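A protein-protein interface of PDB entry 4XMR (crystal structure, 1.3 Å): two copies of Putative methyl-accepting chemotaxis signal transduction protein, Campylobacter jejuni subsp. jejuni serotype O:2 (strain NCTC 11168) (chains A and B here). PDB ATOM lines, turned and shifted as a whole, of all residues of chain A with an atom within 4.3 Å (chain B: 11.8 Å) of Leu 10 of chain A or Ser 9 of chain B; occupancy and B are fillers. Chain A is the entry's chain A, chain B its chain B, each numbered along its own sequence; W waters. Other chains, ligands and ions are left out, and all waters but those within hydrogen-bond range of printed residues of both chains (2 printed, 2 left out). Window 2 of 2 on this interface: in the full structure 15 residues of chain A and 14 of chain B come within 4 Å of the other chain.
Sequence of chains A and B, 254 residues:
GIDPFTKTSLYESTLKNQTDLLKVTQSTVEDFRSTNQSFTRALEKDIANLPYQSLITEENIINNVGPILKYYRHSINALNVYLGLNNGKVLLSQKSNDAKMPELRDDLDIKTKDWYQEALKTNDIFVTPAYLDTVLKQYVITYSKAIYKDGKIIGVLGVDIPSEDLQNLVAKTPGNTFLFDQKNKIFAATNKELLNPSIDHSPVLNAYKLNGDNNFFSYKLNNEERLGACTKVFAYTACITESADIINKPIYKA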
ATOM      1  N   THR A   6     -15.889  -7.407 -23.840  1.00  0.00           N
ATOM      2  CA  THR A   6     -16.188  -8.458 -22.882  1.00  0.00           C
ATOM      3  C   THR A   6     -15.505  -9.771 -23.269  1.00  0.00           C
ATOM      4  O   THR A   6     -14.907 -10.447 -22.423  1.00  0.00           O
ATOM      5  CB  THR A   6     -17.704  -8.653 -22.732  1.00  0.00           C
ATOM      6  OG1 THR A   6     -18.280  -7.436 -22.244  1.00  0.00           O
ATOM      7  CG2 THR A   6     -18.002  -9.775 -21.748  1.00  0.00           C
ATOM      8  N   LYS A   7     -15.563 -10.129 -24.547  1.00  0.00           N
ATOM      9  CA  LYS A   7     -14.898 -11.354 -24.984  1.00  0.00           C
ATOM     10  C   LYS A   7     -13.390 -11.286 -24.743  1.00  0.00           C
ATOM     11  O   LYS A   7     -12.789 -12.251 -24.283  1.00  0.00           O
ATOM     12  CB  LYS A   7     -15.202 -11.679 -26.446  1.00  0.00           C
ATOM     13  CG  LYS A   7     -14.657 -13.040 -26.871  1.00  0.00           C
ATOM     14  CD  LYS A   7     -14.958 -13.358 -28.327  1.00  0.00           C
ATOM     15  CE  LYS A   7     -14.311 -14.677 -28.733  1.00  0.00           C
ATOM     16  NZ  LYS A   7     -14.462 -14.949 -30.190  1.00  0.00           N
ATOM     17  N   THR A   8     -12.786 -10.140 -25.030  1.00  0.00           N
ATOM     18  CA  THR A   8     -11.364  -9.950 -24.762  1.00  0.00           C
ATOM     19  C   THR A   8     -11.048 -10.119 -23.276  1.00  0.00           C
ATOM     20  O   THR A   8     -10.052 -10.748 -22.923  1.00  0.00           O
ATOM     21  CB  THR A   8     -10.856  -8.590 -25.275  1.00  0.00           C
ATOM     22  OG1 THR A   8     -10.948  -8.559 -26.706  1.00  0.00           O
ATOM     23  CG2 THR A   8      -9.405  -8.347 -24.854  1.00  0.00           C
ATOM     24  N   SER A   9     -11.901  -9.595 -22.402  1.00  0.00           N
ATOM     25  CA  SER A   9     -11.677  -9.727 -20.966  1.00  0.00           C
ATOM     26  C   SER A   9     -11.729 -11.191 -20.522  1.00  0.00           C
ATOM     27  O   SER A   9     -10.951 -11.609 -19.675  1.00  0.00           O
ATOM     28  CB  SER A   9     -12.672  -8.875 -20.156  1.00  0.00           C
ATOM     29  OG  SER A   9     -13.968  -9.450 -20.142  1.00  0.00           O
ATOM     30  N   LEU A  10     -12.645 -11.959 -21.105  1.00  0.00           N
ATOM     31  CA  LEU A  10     -12.798 -13.370 -20.766  1.00  0.00           C
ATOM     32  C   LEU A  10     -11.606 -14.160 -21.274  1.00  0.00           C
ATOM     33  O   LEU A  10     -11.080 -15.040 -20.585  1.00  0.00           O
ATOM     34  CB  LEU A  10     -14.077 -13.936 -21.375  1.00  0.00           C
ATOM     35  CG  LEU A  10     -15.366 -13.375 -20.763  1.00  0.00           C
ATOM     36  CD1 LEU A  10     -16.564 -13.726 -21.615  1.00  0.00           C
ATOM     37  CD2 LEU A  10     -15.559 -13.895 -19.356  1.00  0.00           C
ATOM     38  N   TYR A  11     -11.181 -13.842 -22.490  1.00  0.00           N
ATOM     39  CA  TYR A  11     -10.046 -14.508 -23.099  1.00  0.00           C
ATOM     40  C   TYR A  11      -8.760 -14.259 -22.315  1.00  0.00           C
ATOM     41  O   TYR A  11      -8.025 -15.204 -21.998  1.00  0.00           O
ATOM     42  CB  TYR A  11      -9.881 -14.043 -24.542  1.00  0.00           C
ATOM     43  CG  TYR A  11      -8.708 -14.699 -25.228  1.00  0.00           C
ATOM     44  CD1 TYR A  11      -8.800 -16.001 -25.712  1.00  0.00           C
ATOM     45  CD2 TYR A  11      -7.505 -14.024 -25.387  1.00  0.00           C
ATOM     46  CE1 TYR A  11      -7.723 -16.612 -26.340  1.00  0.00           C
ATOM     47  CE2 TYR A  11      -6.425 -14.625 -26.012  1.00  0.00           C
ATOM     48  CZ  TYR A  11      -6.542 -15.915 -26.483  1.00  0.00           C
ATOM     49  OH  TYR A  11      -5.471 -16.503 -27.108  1.00  0.00           O
ATOM     50  N   GLU A  12      -8.494 -12.998 -21.986  1.00  0.00           N
ATOM     51  CA  GLU A  12      -7.262 -12.657 -21.281  1.00  0.00           C
ATOM     52  C   GLU A  12      -7.226 -13.282 -19.890  1.00  0.00           C
ATOM     53  O   GLU A  12      -6.171 -13.735 -19.427  1.00  0.00           O
ATOM     54  CB  GLU A  12      -7.047 -11.139 -21.239  1.00  0.00           C
ATOM     55  CG  GLU A  12      -6.804 -10.553 -22.620  1.00  0.00           C
ATOM     56  CD  GLU A  12      -6.414  -9.093 -22.593  1.00  0.00           C
ATOM     57  OE1 GLU A  12      -6.407  -8.494 -21.499  1.00  0.00           O
ATOM     58  OE2 GLU A  12      -6.111  -8.542 -23.675  1.00  0.00           O
ATOM     59  N   SER A  13      -8.384 -13.333 -19.239  1.00  0.00           N
ATOM     60  CA  SER A  13      -8.514 -13.964 -17.932  1.00  0.00           C
ATOM     61  C   SER A  13      -8.249 -15.471 -18.005  1.00  0.00           C
ATOM     62  O   SER A  13      -7.476 -16.004 -17.209  1.00  0.00           O
ATOM     63  CB  SER A  13      -9.899 -13.701 -17.333  1.00  0.00           C
ATOM     64  OG  SER A  13     -10.030 -14.310 -16.060  1.00  0.00           O
ATOM     65  N   THR A  14      -8.885 -16.164 -18.946  1.00  0.00           N
ATOM     66  CA  THR A  14      -8.728 -17.608 -18.996  1.00  0.00           C
ATOM     67  C   THR A  14      -7.329 -17.985 -19.482  1.00  0.00           C
ATOM     68  O   THR A  14      -6.759 -18.981 -19.034  1.00  0.00           O
ATOM     69  CB  THR A  14      -9.835 -18.315 -19.820  1.00  0.00           C
ATOM     70  OG1 THR A  14      -9.812 -19.718 -19.524  1.00  0.00           O
ATOM     71  CG2 THR A  14      -9.655 -18.103 -21.321  1.00  0.00           C
ATOM     72  N   ILE A 246     -16.129 -20.740 -22.181  1.00  0.00           N
ATOM     73  CA  ILE A 246     -15.839 -19.654 -21.256  1.00  0.00           C
ATOM     74  C   ILE A 246     -15.765 -18.287 -21.956  1.00  0.00           C
ATOM     75  O   ILE A 246     -16.180 -17.270 -21.394  1.00  0.00           O
ATOM     76  CB  ILE A 246     -14.553 -19.962 -20.429  1.00  0.00           C
ATOM     77  CG1 ILE A 246     -14.410 -18.997 -19.251  1.00  0.00           C
ATOM     78  CG2 ILE A 246     -13.303 -19.975 -21.312  1.00  0.00           C
ATOM     79  CD1 ILE A 246     -13.337 -19.422 -18.268  1.00  0.00           C
ATOM     80  N   ILE A 247     -15.279 -18.264 -23.196  1.00  0.00           N
ATOM     81  CA  ILE A 247     -15.219 -17.013 -23.953  1.00  0.00           C
ATOM     82  C   ILE A 247     -16.380 -16.821 -24.932  1.00  0.00           C
ATOM     83  O   ILE A 247     -16.697 -15.692 -25.301  1.00  0.00           O
ATOM     84  CB  ILE A 247     -13.885 -16.836 -24.714  1.00  0.00           C
ATOM     85  CG1 ILE A 247     -13.785 -17.817 -25.887  1.00  0.00           C
ATOM     86  CG2 ILE A 247     -12.691 -16.980 -23.762  1.00  0.00           C
ATOM     87  CD1 ILE A 247     -12.550 -17.617 -26.736  1.00  0.00           C
ATOM     88  N   ASP B   3     -23.344  -6.309  -5.693  1.00  0.00           N
ATOM     89  CA  ASP B   3     -22.430  -5.819  -6.724  1.00  0.00           C
ATOM     90  C   ASP B   3     -22.724  -6.534  -8.042  1.00  0.00           C
ATOM     91  O   ASP B   3     -22.574  -7.746  -8.135  1.00  0.00           O
ATOM     92  CB  ASP B   3     -20.994  -6.097  -6.261  1.00  0.00           C
ATOM     93  CG  ASP B   3     -19.937  -5.663  -7.267  1.00  0.00           C
ATOM     94  OD1 ASP B   3     -20.280  -5.242  -8.387  1.00  0.00           O
ATOM     95  OD2 ASP B   3     -18.737  -5.769  -6.924  1.00  0.00           O
ATOM     96  N   PRO B   4     -23.141  -5.783  -9.073  1.00  0.00           N
ATOM     97  CA  PRO B   4     -23.513  -6.457 -10.325  1.00  0.00           C
ATOM     98  C   PRO B   4     -22.387  -7.303 -10.936  1.00  0.00           C
ATOM     99  O   PRO B   4     -22.659  -8.282 -11.640  1.00  0.00           O
ATOM    100  CB  PRO B   4     -23.890  -5.290 -11.249  1.00  0.00           C
ATOM    101  CG  PRO B   4     -24.406  -4.232 -10.287  1.00  0.00           C
ATOM    102  CD  PRO B   4     -23.469  -4.342  -9.101  1.00  0.00           C
ATOM    103  N   PHE B   5     -21.139  -6.948 -10.653  1.00  0.00           N
ATOM    104  CA  PHE B   5     -20.036  -7.690 -11.240  1.00  0.00           C
ATOM    105  C   PHE B   5     -20.015  -9.122 -10.728  1.00  0.00           C
ATOM    106  O   PHE B   5     -19.542 -10.026 -11.421  1.00  0.00           O
ATOM    107  CB  PHE B   5     -18.691  -7.014 -10.973  1.00  0.00           C
ATOM    108  CG  PHE B   5     -17.558  -7.613 -11.759  1.00  0.00           C
ATOM    109  CD1 PHE B   5     -17.466  -7.412 -13.133  1.00  0.00           C
ATOM    110  CD2 PHE B   5     -16.587  -8.374 -11.132  1.00  0.00           C
ATOM    111  CE1 PHE B   5     -16.426  -7.974 -13.865  1.00  0.00           C
ATOM    112  CE2 PHE B   5     -15.548  -8.938 -11.859  1.00  0.00           C
ATOM    113  CZ  PHE B   5     -15.469  -8.730 -13.222  1.00  0.00           C
ATOM    114  N   THR B   6     -20.521  -9.331  -9.519  1.00  0.00           N
ATOM    115  CA  THR B   6     -20.532 -10.669  -8.937  1.00  0.00           C
ATOM    116  C   THR B   6     -21.454 -11.652  -9.655  1.00  0.00           C
ATOM    117  O   THR B   6     -21.399 -12.857  -9.396  1.00  0.00           O
ATOM    118  CB  THR B   6     -20.868 -10.657  -7.433  1.00  0.00           C
ATOM    119  OG1 THR B   6     -22.228 -10.256  -7.244  1.00  0.00           O
ATOM    120  CG2 THR B   6     -19.936  -9.713  -6.686  1.00  0.00           C
ATOM    121  N   LYS B   7     -22.289 -11.141 -10.556  1.00  0.00           N
ATOM    122  CA  LYS B   7     -23.179 -11.985 -11.345  1.00  0.00           C
ATOM    123  C   LYS B   7     -22.592 -12.371 -12.696  1.00  0.00           C
ATOM    124  O   LYS B   7     -23.236 -13.074 -13.475  1.00  0.00           O
ATOM    125  CB  LYS B   7     -24.524 -11.286 -11.558  1.00  0.00           C
ATOM    126  CG  LYS B   7     -25.206 -10.925 -10.261  1.00  0.00           C
ATOM    127  CD  LYS B   7     -26.552 -10.260 -10.486  1.00  0.00           C
ATOM    128  CE  LYS B   7     -26.998  -9.571  -9.209  1.00  0.00           C
ATOM    129  NZ  LYS B   7     -28.473  -9.548  -9.046  1.00  0.00           N
ATOM    130  N   THR B   8     -21.371 -11.923 -12.975  1.00  0.00           N
ATOM    131  CA  THR B   8     -20.751 -12.200 -14.274  1.00  0.00           C
ATOM    132  C   THR B   8     -20.013 -13.535 -14.305  1.00  0.00           C
ATOM    133  O   THR B   8     -19.523 -14.024 -13.281  1.00  0.00           O
ATOM    134  CB  THR B   8     -19.757 -11.102 -14.712  1.00  0.00           C
ATOM    135  OG1 THR B   8     -18.622 -11.098 -13.837  1.00  0.00           O
ATOM    136  CG2 THR B   8     -20.418  -9.718 -14.740  1.00  0.00           C
ATOM    137  N   SER B   9     -19.918 -14.107 -15.497  1.00  0.00           N
ATOM    138  CA  SER B   9     -19.142 -15.322 -15.689  1.00  0.00           C
ATOM    139  C   SER B   9     -17.648 -15.064 -15.437  1.00  0.00           C
ATOM    140  O   SER B   9     -16.919 -15.946 -14.974  1.00  0.00           O
ATOM    141  CB  SER B   9     -19.372 -15.891 -17.092  1.00  0.00           C
ATOM    142  OG  SER B   9     -18.802 -15.057 -18.082  1.00  0.00           O
ATOM    143  N   LEU B  10     -17.196 -13.846 -15.722  1.00  0.00           N
ATOM    144  CA  LEU B  10     -15.807 -13.494 -15.467  1.00  0.00           C
ATOM    145  C   LEU B  10     -15.501 -13.547 -13.976  1.00  0.00           C
ATOM    146  O   LEU B  10     -14.477 -14.093 -13.572  1.00  0.00           O
ATOM    147  CB  LEU B  10     -15.478 -12.120 -16.044  1.00  0.00           C
ATOM    148  CG  LEU B  10     -14.079 -11.583 -15.749  1.00  0.00           C
ATOM    149  CD1 LEU B  10     -13.012 -12.574 -16.206  1.00  0.00           C
ATOM    150  CD2 LEU B  10     -13.880 -10.223 -16.418  1.00  0.00           C
ATOM    151  N   TYR B  11     -16.391 -12.997 -13.152  1.00  0.00           N
ATOM    152  CA  TYR B  11     -16.198 -13.067 -11.709  1.00  0.00           C
ATOM    153  C   TYR B  11     -16.176 -14.513 -11.232  1.00  0.00           C
ATOM    154  O   TYR B  11     -15.319 -14.900 -10.430  1.00  0.00           O
ATOM    155  CB  TYR B  11     -17.311 -12.304 -11.000  1.00  0.00           C
ATOM    156  CG  TYR B  11     -17.177 -12.242  -9.492  1.00  0.00           C
ATOM    157  CD1 TYR B  11     -16.343 -11.307  -8.892  1.00  0.00           C
ATOM    158  CD2 TYR B  11     -17.914 -13.090  -8.674  1.00  0.00           C
ATOM    159  CE1 TYR B  11     -16.232 -11.223  -7.523  1.00  0.00           C
ATOM    160  CE2 TYR B  11     -17.816 -13.016  -7.301  1.00  0.00           C
ATOM    161  CZ  TYR B  11     -16.971 -12.083  -6.731  1.00  0.00           C
ATOM    162  OH  TYR B  11     -16.869 -11.998  -5.365  1.00  0.00           O
ATOM    163  N   GLU B  12     -17.111 -15.309 -11.733  1.00  0.00           N
ATOM    164  CA  GLU B  12     -17.222 -16.709 -11.333  1.00  0.00           C
ATOM    165  C   GLU B  12     -15.941 -17.473 -11.651  1.00  0.00           C
ATOM    166  O   GLU B  12     -15.421 -18.217 -10.813  1.00  0.00           O
ATOM    167  CB  GLU B  12     -18.417 -17.381 -12.021  1.00  0.00           C
ATOM    168  CG  GLU B  12     -18.584 -18.853 -11.637  1.00  0.00           C
ATOM    169  CD  GLU B  12     -19.630 -19.581 -12.466  1.00  0.00           C
ATOM    170  OE1 GLU B  12     -20.242 -18.951 -13.353  1.00  0.00           O
ATOM    171  OE2 GLU B  12     -19.833 -20.790 -12.232  1.00  0.00           O
ATOM    172  N   SER B  13     -15.430 -17.305 -12.862  1.00  0.00           N
ATOM    173  CA  SER B  13     -14.225 -18.028 -13.234  1.00  0.00           C
ATOM    174  C   SER B  13     -13.039 -17.519 -12.416  1.00  0.00           C
ATOM    175  O   SER B  13     -12.205 -18.310 -11.983  1.00  0.00           O
ATOM    176  CB  SER B  13     -13.957 -17.955 -14.741  1.00  0.00           C
ATOM    177  OG  SER B  13     -13.745 -16.628 -15.175  1.00  0.00           O
ATOM    178  N   THR B  14     -12.987 -16.212 -12.172  1.00  0.00           N
ATOM    179  CA  THR B  14     -11.905 -15.638 -11.383  1.00  0.00           C
ATOM    180  C   THR B  14     -11.834 -16.257  -9.991  1.00  0.00           C
ATOM    181  O   THR B  14     -10.757 -16.599  -9.502  1.00  0.00           O
ATOM    182  CB  THR B  14     -12.070 -14.118 -11.271  1.00  0.00           C
ATOM    183  OG1 THR B  14     -11.964 -13.541 -12.581  1.00  0.00           O
ATOM    184  CG2 THR B  14     -11.007 -13.521 -10.362  1.00  0.00           C
ATOM    185  N   LEU B  15     -12.982 -16.437  -9.357  1.00  0.00           N
ATOM    186  CA  LEU B  15     -12.989 -17.060  -8.043  1.00  0.00           C
ATOM    187  C   LEU B  15     -12.613 -18.543  -8.122  1.00  0.00           C
ATOM    188  O   LEU B  15     -11.938 -19.057  -7.239  1.00  0.00           O
ATOM    189  CB  LEU B  15     -14.330 -16.853  -7.339  1.00  0.00           C
ATOM    190  CG  LEU B  15     -14.410 -15.577  -6.472  1.00  0.00           C
ATOM    191  CD1 LEU B  15     -14.094 -14.308  -7.250  1.00  0.00           C
ATOM    192  CD2 LEU B  15     -15.767 -15.473  -5.785  1.00  0.00           C
ATOM    193  N   LYS B  16     -13.050 -19.220  -9.177  1.00  0.00           N
ATOM    194  CA  LYS B  16     -12.682 -20.613  -9.375  1.00  0.00           C
ATOM    195  C   LYS B  16     -11.162 -20.738  -9.478  1.00  0.00           C
ATOM    196  O   LYS B  16     -10.557 -21.645  -8.911  1.00  0.00           O
ATOM    197  CB  LYS B  16     -13.370 -21.177 -10.621  1.00  0.00           C
ATOM    198  CG  LYS B  16     -12.921 -22.586 -11.003  1.00  0.00           C
ATOM    199  CD  LYS B  16     -13.795 -23.153 -12.115  1.00  0.00           C
ATOM    200  CE  LYS B  16     -12.969 -23.861 -13.177  1.00  0.00           C
ATOM    201  NZ  LYS B  16     -12.177 -24.987 -12.613  1.00  0.00           N
ATOM    202  N   ASN B  17     -10.530 -19.831 -10.213  1.00  0.00           N
ATOM    203  CA  ASN B  17      -9.083 -19.898 -10.335  1.00  0.00           C
ATOM    204  C   ASN B  17      -8.387 -19.579  -9.016  1.00  0.00           C
ATOM    205  O   ASN B  17      -7.433 -20.267  -8.647  1.00  0.00           O
ATOM    206  CB  ASN B  17      -8.552 -19.013 -11.463  1.00  0.00           C
ATOM    207  CG  ASN B  17      -7.080 -19.290 -11.769  1.00  0.00           C
ATOM    208  OD1 ASN B  17      -6.729 -20.335 -12.328  1.00  0.00           O
ATOM    209  ND2 ASN B  17      -6.213 -18.356 -11.395  1.00  0.00           N
ATOM    210  N   GLN B  18      -8.864 -18.565  -8.298  1.00  0.00           N
ATOM    211  CA  GLN B  18      -8.272 -18.265  -6.994  1.00  0.00           C
ATOM    212  C   GLN B  18      -8.392 -19.466  -6.062  1.00  0.00           C
ATOM    213  O   GLN B  18      -7.459 -19.775  -5.319  1.00  0.00           O
ATOM    214  CB  GLN B  18      -8.908 -17.031  -6.354  1.00  0.00           C
ATOM    215  CG  GLN B  18      -8.613 -15.731  -7.099  1.00  0.00           C
ATOM    216  CD  GLN B  18      -7.137 -15.382  -7.074  1.00  0.00           C
ATOM    217  OE1 GLN B  18      -6.401 -15.688  -8.010  1.00  0.00           O
ATOM    218  NE2 GLN B  18      -6.698 -14.742  -5.999  1.00  0.00           N
ATOM    219  N   ILE B 246      -8.195  -5.686  -9.219  1.00  0.00           N
ATOM    220  CA  ILE B 246      -7.664  -6.701 -10.120  1.00  0.00           C
ATOM    221  C   ILE B 246      -8.750  -7.732 -10.414  1.00  0.00           C
ATOM    222  O   ILE B 246      -8.888  -8.204 -11.545  1.00  0.00           O
ATOM    223  CB  ILE B 246      -6.373  -7.346  -9.572  1.00  0.00           C
ATOM    224  CG1 ILE B 246      -5.219  -6.344  -9.663  1.00  0.00           C
ATOM    225  CG2 ILE B 246      -6.026  -8.607 -10.350  1.00  0.00           C
ATOM    226  CD1 ILE B 246      -3.922  -6.835  -9.081  1.00  0.00           C
ATOM    227  N   ILE B 247      -9.543  -8.054  -9.395  1.00  0.00           N
ATOM    228  CA  ILE B 247     -10.692  -8.940  -9.575  1.00  0.00           C
ATOM    229  C   ILE B 247     -11.671  -8.329 -10.594  1.00  0.00           C
ATOM    230  O   ILE B 247     -12.154  -9.004 -11.510  1.00  0.00           O
ATOM    231  CB  ILE B 247     -11.419  -9.200  -8.230  1.00  0.00           C
ATOM    232  CG1 ILE B 247     -10.489  -9.918  -7.225  1.00  0.00           C
ATOM    233  CG2 ILE B 247     -12.734  -9.954  -8.468  1.00  0.00           C
ATOM    234  CD1 ILE B 247     -10.052 -11.304  -7.655  1.00  0.00           C
ATOM    235  N   ASN B 248     -11.932  -7.034 -10.428  1.00  0.00           N
ATOM    236  CA  ASN B 248     -12.828  -6.286 -11.304  1.00  0.00           C
ATOM    237  C   ASN B 248     -12.057  -5.067 -11.771  1.00  0.00           C
ATOM    238  O   ASN B 248     -11.993  -4.055 -11.076  1.00  0.00           O
ATOM    239  CB  ASN B 248     -14.087  -5.855 -10.537  1.00  0.00           C
ATOM    240  CG  ASN B 248     -15.058  -5.062 -11.386  1.00  0.00           C
ATOM    241  OD1 ASN B 248     -14.821  -4.826 -12.570  1.00  0.00           O
ATOM    242  ND2 ASN B 248     -16.164  -4.640 -10.779  1.00  0.00           N
ATOM    243  N   LYS B 249     -11.431  -5.182 -12.937  1.00  0.00           N
ATOM    244  CA  LYS B 249     -10.567  -4.121 -13.434  1.00  0.00           C
ATOM    245  C   LYS B 249     -11.381  -2.916 -13.885  1.00  0.00           C
ATOM    246  O   LYS B 249     -12.137  -3.017 -14.826  1.00  0.00           O
ATOM    247  CB  LYS B 249      -9.740  -4.656 -14.599  1.00  0.00           C
ATOM    248  CG  LYS B 249      -8.770  -3.662 -15.161  1.00  0.00           C
ATOM    249  CD  LYS B 249      -8.017  -4.209 -16.359  1.00  0.00           C
ATOM    250  CE  LYS B 249      -7.436  -3.081 -17.203  1.00  0.00           C
ATOM    251  NZ  LYS B 249      -6.412  -2.282 -16.475  1.00  0.00           N
HETATM  252  O   HOH W   1      -9.084 -14.756 -13.302  1.00  0.00           O
HETATM  253  O   HOH W   2     -11.166 -16.623 -16.195  1.00  0.00           O
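The backbone carbonyl oxygen (O) of Leu 10 of chain B sits at hydrogen-bond distance from the side-chain hydroxyl (OG1) of Thr 14 of chain B (2.8 Å).
The side-chain hydroxyl (OG) of Ser 13 of chain B is in hydrogen-bond range of the backbone carbonyl oxygen (O) of Ser 9 of chain B, 3.3 Å away.
The backbone carbonyl oxygen of Leu 10 of chain B lies within hydrogen-bond range of the side-chain hydroxyl of Ser 13 of chain B, at 3.1 Å.
The backbone carbonyl oxygen (O) of Thr 6 of chain A sits at hydrogen-bond distance from the side-chain hydroxyl (OG) of Ser 9 of chain A (2.7 Å).
Among the printed residues, pairs that only touch across the chains: Ser 9 of chain A with Leu 10 of chain B (3.8 Å), Leu 10 of chain A with Ser 9 of chain B (3.7 Å), Leu 10 of chain A with Leu 10 of chain B (3.8 Å), Ser 13 of chain A with Leu 10 of chain B (3.5 Å) and Ile 246 of chain A with Ser 13 of chain B (3.9 Å).
Ser 9 of chain A touches Leu 10 of chain B, and with the chains exchanged Leu 10 of chain A touches Ser 9 of chain B.
Leu 10 of chain A touches its own counterpart, Leu 10 of chain B.
Ser 13 of chain A touches Leu 10 of chain B, but with the chains exchanged Leu 10 of chain A does not touch Ser 13 of chain B (5.3 Å).
Ile 246 of chain A touches Ser 13 of chain B, but with the chains exchanged Ser 13 of chain A does not touch Ile 246 of chain B (7.7 Å).
11 positions are printed for both chains.
Water W2 lies within hydrogen-bond range of the side-chain hydroxyl (OG) of Ser 13 of chain A (2.6 Å) and the side-chain hydroxyl (OG) of Ser 13 of chain B (2.8 Å).
Water W1 lies within hydrogen-bond range of the side-chain hydroxyl of Ser 13 of chain A (2.9 Å) and the side-chain hydroxyl of Thr 14 of chain B (3.2 Å).
Of chain B, only Ser 9 and Leu 10 come within 4 Å of Leu 10 of chain A.
Ser 9 of chain B touches one residue of chain A.
No residue of chain B comes within 4 Å of Thr 6 of chain A.
No residue of chain B comes within 4 Å of Thr 8 of chain A.
Printed residues of chain B within 4 Å of Ser 13 of chain A: Leu 10.
No residue of chain B comes within 4 Å of Thr 14 of chain A.
No residue of chain B comes within 4 Å of Ile 247 of chain A.
Printed residues of chain A within 4 Å of Leu 10 of chain B: Ser 9, Leu 10 and Ser 13.
Of the printed residues of chain A, Ser 13 of chain B touches Ile 246.
Printed residues of chain B within 4 Å of Ile 246 of chain A: Ser 13.
Gln 18 of chain B touches none of the printed residues of chain A.
The nearest printed residue of chain A that does not touch Ser 9 of chain B is Ile 246 of chain A (4.8 Å).
Printed residues of chain A that touch a printed residue of chain B: Ser 9, Leu 10, Ser 13 and Ile 246.
Hydrophobic or aromatic side chains of chain A that line the printed part of chain B: Leu 10 and Ile 246.
Printed residues of chain B that touch a printed residue of chain A: Ser 9, Leu 10 and Ser 13.
Hydrophobic or aromatic side chains of chain B within 4 Å of the printed part of chain A: Leu 10.
Among the printed residues, no Asp or Glu carboxylate lies within 4 Å of a Lys or Arg side-chain nitrogen of the other chain.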
